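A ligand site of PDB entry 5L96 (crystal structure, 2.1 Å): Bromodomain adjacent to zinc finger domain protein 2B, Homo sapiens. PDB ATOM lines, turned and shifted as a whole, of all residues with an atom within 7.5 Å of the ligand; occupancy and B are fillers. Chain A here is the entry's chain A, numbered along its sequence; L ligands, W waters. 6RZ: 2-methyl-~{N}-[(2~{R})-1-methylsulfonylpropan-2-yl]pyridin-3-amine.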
ATOM      1  N   ALA A  31     -11.822  28.998  31.143  1.00  0.00           N
ATOM      2  CA  ALA A  31     -10.964  29.159  29.953  1.00  0.00           C
ATOM      3  C   ALA A  31      -9.904  28.070  29.805  1.00  0.00           C
ATOM      4  O   ALA A  31      -9.272  27.951  28.741  1.00  0.00           O
ATOM      5  CB  ALA A  31     -10.284  30.527  29.968  1.00  0.00           C
ATOM      6  N   TRP A  32      -9.698  27.291  30.864  1.00  0.00           N
ATOM      7  CA  TRP A  32      -8.586  26.325  30.906  1.00  0.00           C
ATOM      8  C   TRP A  32      -8.504  25.318  29.742  1.00  0.00           C
ATOM      9  O   TRP A  32      -7.397  24.894  29.382  1.00  0.00           O
ATOM     10  CB  TRP A  32      -8.618  25.547  32.230  1.00  0.00           C
ATOM     11  CG  TRP A  32      -9.880  24.778  32.502  1.00  0.00           C
ATOM     12  CD1 TRP A  32     -10.986  25.239  33.149  1.00  0.00           C
ATOM     13  CD2 TRP A  32     -10.151  23.416  32.151  1.00  0.00           C
ATOM     14  NE1 TRP A  32     -11.934  24.251  33.226  1.00  0.00           N
ATOM     15  CE2 TRP A  32     -11.450  23.121  32.616  1.00  0.00           C
ATOM     16  CE3 TRP A  32      -9.429  22.425  31.484  1.00  0.00           C
ATOM     17  CZ2 TRP A  32     -12.041  21.870  32.438  1.00  0.00           C
ATOM     18  CZ3 TRP A  32     -10.020  21.173  31.306  1.00  0.00           C
ATOM     19  CH2 TRP A  32     -11.318  20.916  31.784  1.00  0.00           C
ATOM     20  N   PRO A  33      -9.645  24.920  29.147  1.00  0.00           N
ATOM     21  CA  PRO A  33      -9.406  23.984  28.038  1.00  0.00           C
ATOM     22  C   PRO A  33      -8.895  24.662  26.767  1.00  0.00           C
ATOM     23  O   PRO A  33      -8.532  23.960  25.824  1.00  0.00           O
ATOM     24  CB  PRO A  33     -10.792  23.356  27.795  1.00  0.00           C
ATOM     25  CG  PRO A  33     -11.633  23.750  28.972  1.00  0.00           C
ATOM     26  CD  PRO A  33     -11.091  25.073  29.408  1.00  0.00           C
ATOM     27  N   PHE A  34      -8.867  25.995  26.741  1.00  0.00           N
ATOM     28  CA  PHE A  34      -8.685  26.714  25.479  1.00  0.00           C
ATOM     29  C   PHE A  34      -7.461  27.626  25.468  1.00  0.00           C
ATOM     30  O   PHE A  34      -7.203  28.340  24.486  1.00  0.00           O
ATOM     31  CB  PHE A  34      -9.947  27.525  25.166  1.00  0.00           C
ATOM     32  CG  PHE A  34     -11.216  26.745  25.349  1.00  0.00           C
ATOM     33  CD1 PHE A  34     -11.559  25.742  24.461  1.00  0.00           C
ATOM     34  CD2 PHE A  34     -12.068  26.993  26.429  1.00  0.00           C
ATOM     35  CE1 PHE A  34     -12.722  24.994  24.630  1.00  0.00           C
ATOM     36  CE2 PHE A  34     -13.231  26.264  26.605  1.00  0.00           C
ATOM     37  CZ  PHE A  34     -13.558  25.265  25.706  1.00  0.00           C
ATOM     38  N   LEU A  35      -6.692  27.602  26.554  1.00  0.00           N
ATOM     39  CA  LEU A  35      -5.582  28.530  26.724  1.00  0.00           C
ATOM     40  C   LEU A  35      -4.449  28.196  25.769  1.00  0.00           C
ATOM     41  O   LEU A  35      -3.846  29.093  25.198  1.00  0.00           O
ATOM     42  CB  LEU A  35      -5.087  28.517  28.169  1.00  0.00           C
ATOM     43  CG  LEU A  35      -6.108  29.042  29.204  1.00  0.00           C
ATOM     44  CD1 LEU A  35      -5.546  28.987  30.610  1.00  0.00           C
ATOM     45  CD2 LEU A  35      -6.566  30.453  28.850  1.00  0.00           C
ATOM     46  N   LEU A  36      -4.181  26.902  25.593  1.00  0.00           N
ATOM     47  CA  LEU A  36      -3.076  26.427  24.774  1.00  0.00           C
ATOM     48  C   LEU A  36      -3.567  25.511  23.651  1.00  0.00           C
ATOM     49  O   LEU A  36      -4.687  24.993  23.733  1.00  0.00           O
ATOM     50  CB  LEU A  36      -2.041  25.688  25.630  1.00  0.00           C
ATOM     51  CG  LEU A  36      -1.313  26.508  26.699  1.00  0.00           C
ATOM     52  CD1 LEU A  36      -0.296  25.629  27.412  1.00  0.00           C
ATOM     53  CD2 LEU A  36      -0.642  27.721  26.067  1.00  0.00           C
ATOM     54  N   PRO A  37      -2.751  25.306  22.602  1.00  0.00           N
ATOM     55  CA  PRO A  37      -3.161  24.376  21.543  1.00  0.00           C
ATOM     56  C   PRO A  37      -3.477  23.002  22.114  1.00  0.00           C
ATOM     57  O   PRO A  37      -2.825  22.572  23.068  1.00  0.00           O
ATOM     58  CB  PRO A  37      -1.938  24.299  20.632  1.00  0.00           C
ATOM     59  CG  PRO A  37      -1.230  25.589  20.870  1.00  0.00           C
ATOM     60  CD  PRO A  37      -1.456  25.935  22.304  1.00  0.00           C
ATOM     61  N   VAL A  38      -4.464  22.320  21.558  1.00  0.00           N
ATOM     62  CA  VAL A  38      -4.695  20.948  21.964  1.00  0.00           C
ATOM     63  C   VAL A  38      -3.450  20.142  21.592  1.00  0.00           C
ATOM     64  O   VAL A  38      -2.961  20.231  20.465  1.00  0.00           O
ATOM     65  CB  VAL A  38      -5.952  20.355  21.302  1.00  0.00           C
ATOM     66  CG1 VAL A  38      -6.014  18.851  21.522  1.00  0.00           C
ATOM     67  CG2 VAL A  38      -7.208  21.039  21.843  1.00  0.00           C
ATOM     68  N   ASN A  39      -2.923  19.404  22.561  1.00  0.00           N
ATOM     69  CA  ASN A  39      -1.718  18.607  22.352  1.00  0.00           C
ATOM     70  C   ASN A  39      -2.015  17.455  21.399  1.00  0.00           C
ATOM     71  O   ASN A  39      -2.672  16.480  21.773  1.00  0.00           O
ATOM     72  CB  ASN A  39      -1.187  18.101  23.689  1.00  0.00           C
ATOM     73  CG  ASN A  39       0.197  17.474  23.580  1.00  0.00           C
ATOM     74  OD1 ASN A  39       0.524  16.834  22.583  1.00  0.00           O
ATOM     75  ND2 ASN A  39       0.993  17.655  24.620  1.00  0.00           N
ATOM     76  N   LEU A  40      -1.508  17.566  20.176  1.00  0.00           N
ATOM     77  CA  LEU A  40      -1.840  16.622  19.120  1.00  0.00           C
ATOM     78  C   LEU A  40      -1.273  15.236  19.390  1.00  0.00           C
ATOM     79  O   LEU A  40      -1.796  14.241  18.894  1.00  0.00           O
ATOM     80  CB  LEU A  40      -1.353  17.120  17.759  1.00  0.00           C
ATOM     81  CG  LEU A  40      -2.025  18.411  17.285  1.00  0.00           C
ATOM     82  CD1 LEU A  40      -1.679  18.703  15.834  1.00  0.00           C
ATOM     83  CD2 LEU A  40      -3.538  18.347  17.475  1.00  0.00           C
ATOM     84  N   LYS A  41      -0.240  15.151  20.195  1.00  0.00           N
ATOM     85  CA  LYS A  41       0.369  13.872  20.486  1.00  0.00           C
ATOM     86  C   LYS A  41      -0.270  13.225  21.682  1.00  0.00           C
ATOM     87  O   LYS A  41      -0.037  12.076  21.975  1.00  0.00           O
ATOM     88  CB  LYS A  41       1.875  14.027  20.737  1.00  0.00           C
ATOM     89  CG  LYS A  41       2.655  14.697  19.614  1.00  0.00           C
ATOM     90  CD  LYS A  41       2.089  14.371  18.236  1.00  0.00           C
ATOM     91  CE  LYS A  41       2.838  15.093  17.117  1.00  0.00           C
ATOM     92  NZ  LYS A  41       1.998  15.292  15.903  1.00  0.00           N
ATOM     93  N   LEU A  42      -1.079  13.983  22.390  1.00  0.00           N
ATOM     94  CA  LEU A  42      -1.706  13.514  23.619  1.00  0.00           C
ATOM     95  C   LEU A  42      -3.158  13.129  23.385  1.00  0.00           C
ATOM     96  O   LEU A  42      -3.681  12.231  24.039  1.00  0.00           O
ATOM     97  CB  LEU A  42      -1.611  14.594  24.705  1.00  0.00           C
ATOM     98  CG  LEU A  42      -2.148  14.345  26.118  1.00  0.00           C
ATOM     99  CD1 LEU A  42      -1.365  15.173  27.124  1.00  0.00           C
ATOM    100  CD2 LEU A  42      -3.632  14.687  26.232  1.00  0.00           C
ATOM    101  N   VAL A  43      -3.818  13.816  22.455  1.00  0.00           N
ATOM    102  CA  VAL A  43      -5.227  13.578  22.219  1.00  0.00           C
ATOM    103  C   VAL A  43      -5.437  12.819  20.923  1.00  0.00           C
ATOM    104  O   VAL A  43      -5.264  13.371  19.838  1.00  0.00           O
ATOM    105  CB  VAL A  43      -6.037  14.897  22.167  1.00  0.00           C
ATOM    106  CG1 VAL A  43      -7.516  14.605  22.066  1.00  0.00           C
ATOM    107  CG2 VAL A  43      -5.743  15.741  23.395  1.00  0.00           C
ATOM    108  N   TYR A  46      -7.482  14.030  17.294  1.00  0.00           N
ATOM    109  CA  TYR A  46      -7.709  15.471  17.133  1.00  0.00           C
ATOM    110  C   TYR A  46      -7.135  15.983  15.817  1.00  0.00           C
ATOM    111  O   TYR A  46      -7.803  16.725  15.095  1.00  0.00           O
ATOM    112  CB  TYR A  46      -7.121  16.264  18.294  1.00  0.00           C
ATOM    113  CG  TYR A  46      -7.792  17.608  18.461  1.00  0.00           C
ATOM    114  CD1 TYR A  46      -7.223  18.766  17.934  1.00  0.00           C
ATOM    115  CD2 TYR A  46      -9.023  17.709  19.089  1.00  0.00           C
ATOM    116  CE1 TYR A  46      -7.856  20.003  18.071  1.00  0.00           C
ATOM    117  CE2 TYR A  46      -9.660  18.931  19.236  1.00  0.00           C
ATOM    118  CZ  TYR A  46      -9.080  20.075  18.722  1.00  0.00           C
ATOM    119  OH  TYR A  46      -9.717  21.278  18.862  1.00  0.00           O
ATOM    120  N   ILE A  50     -10.043  17.455  13.383  1.00  0.00           N
ATOM    121  CA  ILE A  50     -10.185  18.913  13.412  1.00  0.00           C
ATOM    122  C   ILE A  50      -9.221  19.568  12.434  1.00  0.00           C
ATOM    123  O   ILE A  50      -8.012  19.637  12.688  1.00  0.00           O
ATOM    124  CB  ILE A  50      -9.941  19.489  14.834  1.00  0.00           C
ATOM    125  CG1 ILE A  50     -10.890  18.830  15.852  1.00  0.00           C
ATOM    126  CG2 ILE A  50     -10.108  21.018  14.844  1.00  0.00           C
ATOM    127  CD1 ILE A  50     -12.342  19.168  15.643  1.00  0.00           C
ATOM    128  N   MET A  54      -7.524  25.818  16.913  1.00  0.00           N
ATOM    129  CA  MET A  54      -7.344  27.196  17.350  1.00  0.00           C
ATOM    130  C   MET A  54      -7.476  27.242  18.875  1.00  0.00           C
ATOM    131  O   MET A  54      -8.149  26.403  19.467  1.00  0.00           O
ATOM    132  CB  MET A  54      -8.353  28.119  16.661  1.00  0.00           C
ATOM    133  CG  MET A  54      -8.155  29.620  16.923  1.00  0.00           C
ATOM    134  SD  MET A  54      -6.522  30.201  16.424  1.00  0.00           S
ATOM    135  CE  MET A  54      -6.530  29.794  14.673  1.00  0.00           C
ATOM    136  N   VAL A  81     -12.612  28.258  17.862  1.00  0.00           N
ATOM    137  CA  VAL A  81     -12.293  27.566  19.117  1.00  0.00           C
ATOM    138  C   VAL A  81     -13.485  26.766  19.651  1.00  0.00           C
ATOM    139  O   VAL A  81     -13.352  25.589  20.006  1.00  0.00           O
ATOM    140  CB  VAL A  81     -11.854  28.560  20.204  1.00  0.00           C
ATOM    141  CG1 VAL A  81     -11.741  27.849  21.564  1.00  0.00           C
ATOM    142  CG2 VAL A  81     -10.520  29.235  19.830  1.00  0.00           C
ATOM    143  N   ASN A  84     -14.767  23.988  17.114  1.00  0.00           N
ATOM    144  CA  ASN A  84     -13.925  22.801  17.270  1.00  0.00           C
ATOM    145  C   ASN A  84     -14.285  22.052  18.547  1.00  0.00           C
ATOM    146  O   ASN A  84     -14.316  20.819  18.561  1.00  0.00           O
ATOM    147  CB  ASN A  84     -12.440  23.183  17.297  1.00  0.00           C
ATOM    148  CG  ASN A  84     -11.940  23.742  15.975  1.00  0.00           C
ATOM    149  OD1 ASN A  84     -12.556  23.536  14.925  1.00  0.00           O
ATOM    150  ND2 ASN A  84     -10.801  24.440  16.012  1.00  0.00           N
ATOM    151  N   CYS A  85     -14.572  22.792  19.617  1.00  0.00           N
ATOM    152  CA  CYS A  85     -14.870  22.157  20.892  1.00  0.00           C
ATOM    153  C   CYS A  85     -16.155  21.335  20.800  1.00  0.00           C
ATOM    154  O   CYS A  85     -16.208  20.216  21.312  1.00  0.00           O
ATOM    155  CB  CYS A  85     -14.972  23.199  22.018  1.00  0.00           C
ATOM    156  SG  CYS A  85     -15.319  22.496  23.678  1.00  0.00           S
ATOM    157  N   GLU A  86     -17.175  21.871  20.129  1.00  0.00           N
ATOM    158  CA  GLU A  86     -18.455  21.172  19.988  1.00  0.00           C
ATOM    159  C   GLU A  86     -18.327  19.933  19.119  1.00  0.00           C
ATOM    160  O   GLU A  86     -19.035  18.956  19.323  1.00  0.00           O
ATOM    161  CB  GLU A  86     -19.521  22.091  19.377  1.00  0.00           C
ATOM    162  CG  GLU A  86     -20.267  22.938  20.370  1.00  0.00           C
ATOM    163  CD  GLU A  86     -21.561  23.480  19.799  1.00  0.00           C
ATOM    164  OE1 GLU A  86     -21.727  24.727  19.766  1.00  0.00           O
ATOM    165  OE2 GLU A  86     -22.402  22.673  19.374  1.00  0.00           O
ATOM    166  N   PHE A  88     -15.704  17.924  18.958  1.00  0.00           N
ATOM    167  CA  PHE A  88     -14.909  16.860  19.557  1.00  0.00           C
ATOM    168  C   PHE A  88     -15.408  16.401  20.928  1.00  0.00           C
ATOM    169  O   PHE A  88     -15.162  15.260  21.317  1.00  0.00           O
ATOM    170  CB  PHE A  88     -13.439  17.316  19.675  1.00  0.00           C
ATOM    171  CG  PHE A  88     -12.453  16.168  19.675  1.00  0.00           C
ATOM    172  CD1 PHE A  88     -12.090  15.554  18.480  1.00  0.00           C
ATOM    173  CD2 PHE A  88     -11.899  15.714  20.860  1.00  0.00           C
ATOM    174  CE1 PHE A  88     -11.179  14.507  18.470  1.00  0.00           C
ATOM    175  CE2 PHE A  88     -10.987  14.667  20.849  1.00  0.00           C
ATOM    176  CZ  PHE A  88     -10.633  14.051  19.660  1.00  0.00           C
ATOM    177  N   ASN A  89     -16.094  17.265  21.650  1.00  0.00           N
ATOM    178  CA  ASN A  89     -16.492  16.962  23.019  1.00  0.00           C
ATOM    179  C   ASN A  89     -18.013  16.868  23.204  1.00  0.00           C
ATOM    180  O   ASN A  89     -18.762  17.620  22.584  1.00  0.00           O
ATOM    181  CB  ASN A  89     -15.945  18.028  23.977  1.00  0.00           C
ATOM    182  CG  ASN A  89     -14.441  18.235  23.834  1.00  0.00           C
ATOM    183  OD1 ASN A  89     -13.648  17.555  24.487  1.00  0.00           O
ATOM    184  ND2 ASN A  89     -14.032  19.184  22.984  1.00  0.00           N
ATOM    185  N   ILE A  95     -15.221  19.721  29.416  1.00  0.00           N
ATOM    186  CA  ILE A  95     -14.699  20.555  28.336  1.00  0.00           C
ATOM    187  C   ILE A  95     -15.827  21.058  27.434  1.00  0.00           C
ATOM    188  O   ILE A  95     -15.832  22.216  27.030  1.00  0.00           O
ATOM    189  CB  ILE A  95     -13.672  19.789  27.478  1.00  0.00           C
ATOM    190  CG1 ILE A  95     -12.412  19.477  28.304  1.00  0.00           C
ATOM    191  CG2 ILE A  95     -13.313  20.581  26.231  1.00  0.00           C
ATOM    192  CD1 ILE A  95     -11.424  18.581  27.608  1.00  0.00           C
ATOM    193  N   GLY A  96     -16.783  20.187  27.147  1.00  0.00           N
ATOM    194  CA  GLY A  96     -17.917  20.537  26.321  1.00  0.00           C
ATOM    195  C   GLY A  96     -18.768  21.684  26.857  1.00  0.00           C
ATOM    196  O   GLY A  96     -19.130  22.591  26.115  1.00  0.00           O
HETATM  197  C13 6RZ L   1     -10.559  18.513  22.663  1.00  0.00           C
HETATM  198  C15 6RZ L   1      -9.028  18.453  24.562  1.00  0.00           C
HETATM  199  C01 6RZ L   1      -7.430  20.820  27.789  1.00  0.00           C
HETATM  200  C05 6RZ L   1      -6.006  17.455  26.625  1.00  0.00           C
HETATM  201  N08 6RZ L   1      -8.617  20.611  25.744  1.00  0.00           N
HETATM  202  C09 6RZ L   1      -9.246  19.839  24.711  1.00  0.00           C
HETATM  203  C02 6RZ L   1      -7.565  20.082  26.485  1.00  0.00           C
HETATM  204  C03 6RZ L   1      -6.249  20.207  25.684  1.00  0.00           C
HETATM  205  S04 6RZ L   1      -5.127  18.892  26.209  1.00  0.00           S
HETATM  206  O06 6RZ L   1      -4.116  18.627  25.162  1.00  0.00           O
HETATM  207  O07 6RZ L   1      -4.279  19.362  27.357  1.00  0.00           O
HETATM  208  C10 6RZ L   1     -10.138  20.465  23.799  1.00  0.00           C
HETATM  209  C11 6RZ L   1     -10.409  21.962  23.937  1.00  0.00           C
HETATM  210  N12 6RZ L   1     -10.754  19.805  22.837  1.00  0.00           N
HETATM  211  C14 6RZ L   1      -9.693  17.785  23.505  1.00  0.00           C
HETATM  212  O   HOH W   1     -11.553  21.290  20.664  1.00  0.00           O
HETATM  213  O   HOH W   2      -3.737  22.190  26.026  1.00  0.00           O
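The side-chain amide nitrogen (ND2) of Asn 89 lies within hydrogen-bond range of a nitrogen (N12) of the ligand (3.3 Å).
An oxygen (O06) of the ligand is in hydrogen-bond range of the backbone NH (N) of Asn 39 (3.0 Å).
N08 of the ligand lies close to O of Pro 33 (3.4 Å).
SG of Cys 85 sits at hydrogen-bond distance from O of Ile 95 (3.4 Å).
The side-chain amide oxygen (OD1) of Asn 39 sits at hydrogen-bond distance from the backbone NH (N) of Lys 41.
N of Leu 42 sits at hydrogen-bond distance from OD1 of Asn 39 (3.3 Å).
ND2 of Asn 89 sits at hydrogen-bond distance from O of Cys 85 (2.9 Å).
CE1 of Phe 34 touches C11 of the ligand (3.9 Å).
CG2 of Val 38 touches C10 of the ligand, 3.6 Å away.
Leu 42 touches the ligand (CD2 to C05, 3.7 Å).
Val 43 touches the ligand (CG2 to C05, 3.7 Å).
CE2 of Tyr 46 touches C13 of the ligand, 3.6 Å away.
Phe 88 touches the ligand.
Ile 95 touches the ligand.
Hydrophobic or aromatic side chains that line the ligand: Phe 34, Val 38, Leu 42, Val 43, Tyr 46, Phe 88 and Ile 95.
Water W1 lies within hydrogen-bond range of the side-chain hydroxyl (OH) of Tyr 46 and a nitrogen (N12) of the ligand.
Water W2 bridges the backbone carbonyl oxygen of Pro 37 and an oxygen (O07) of the ligand.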
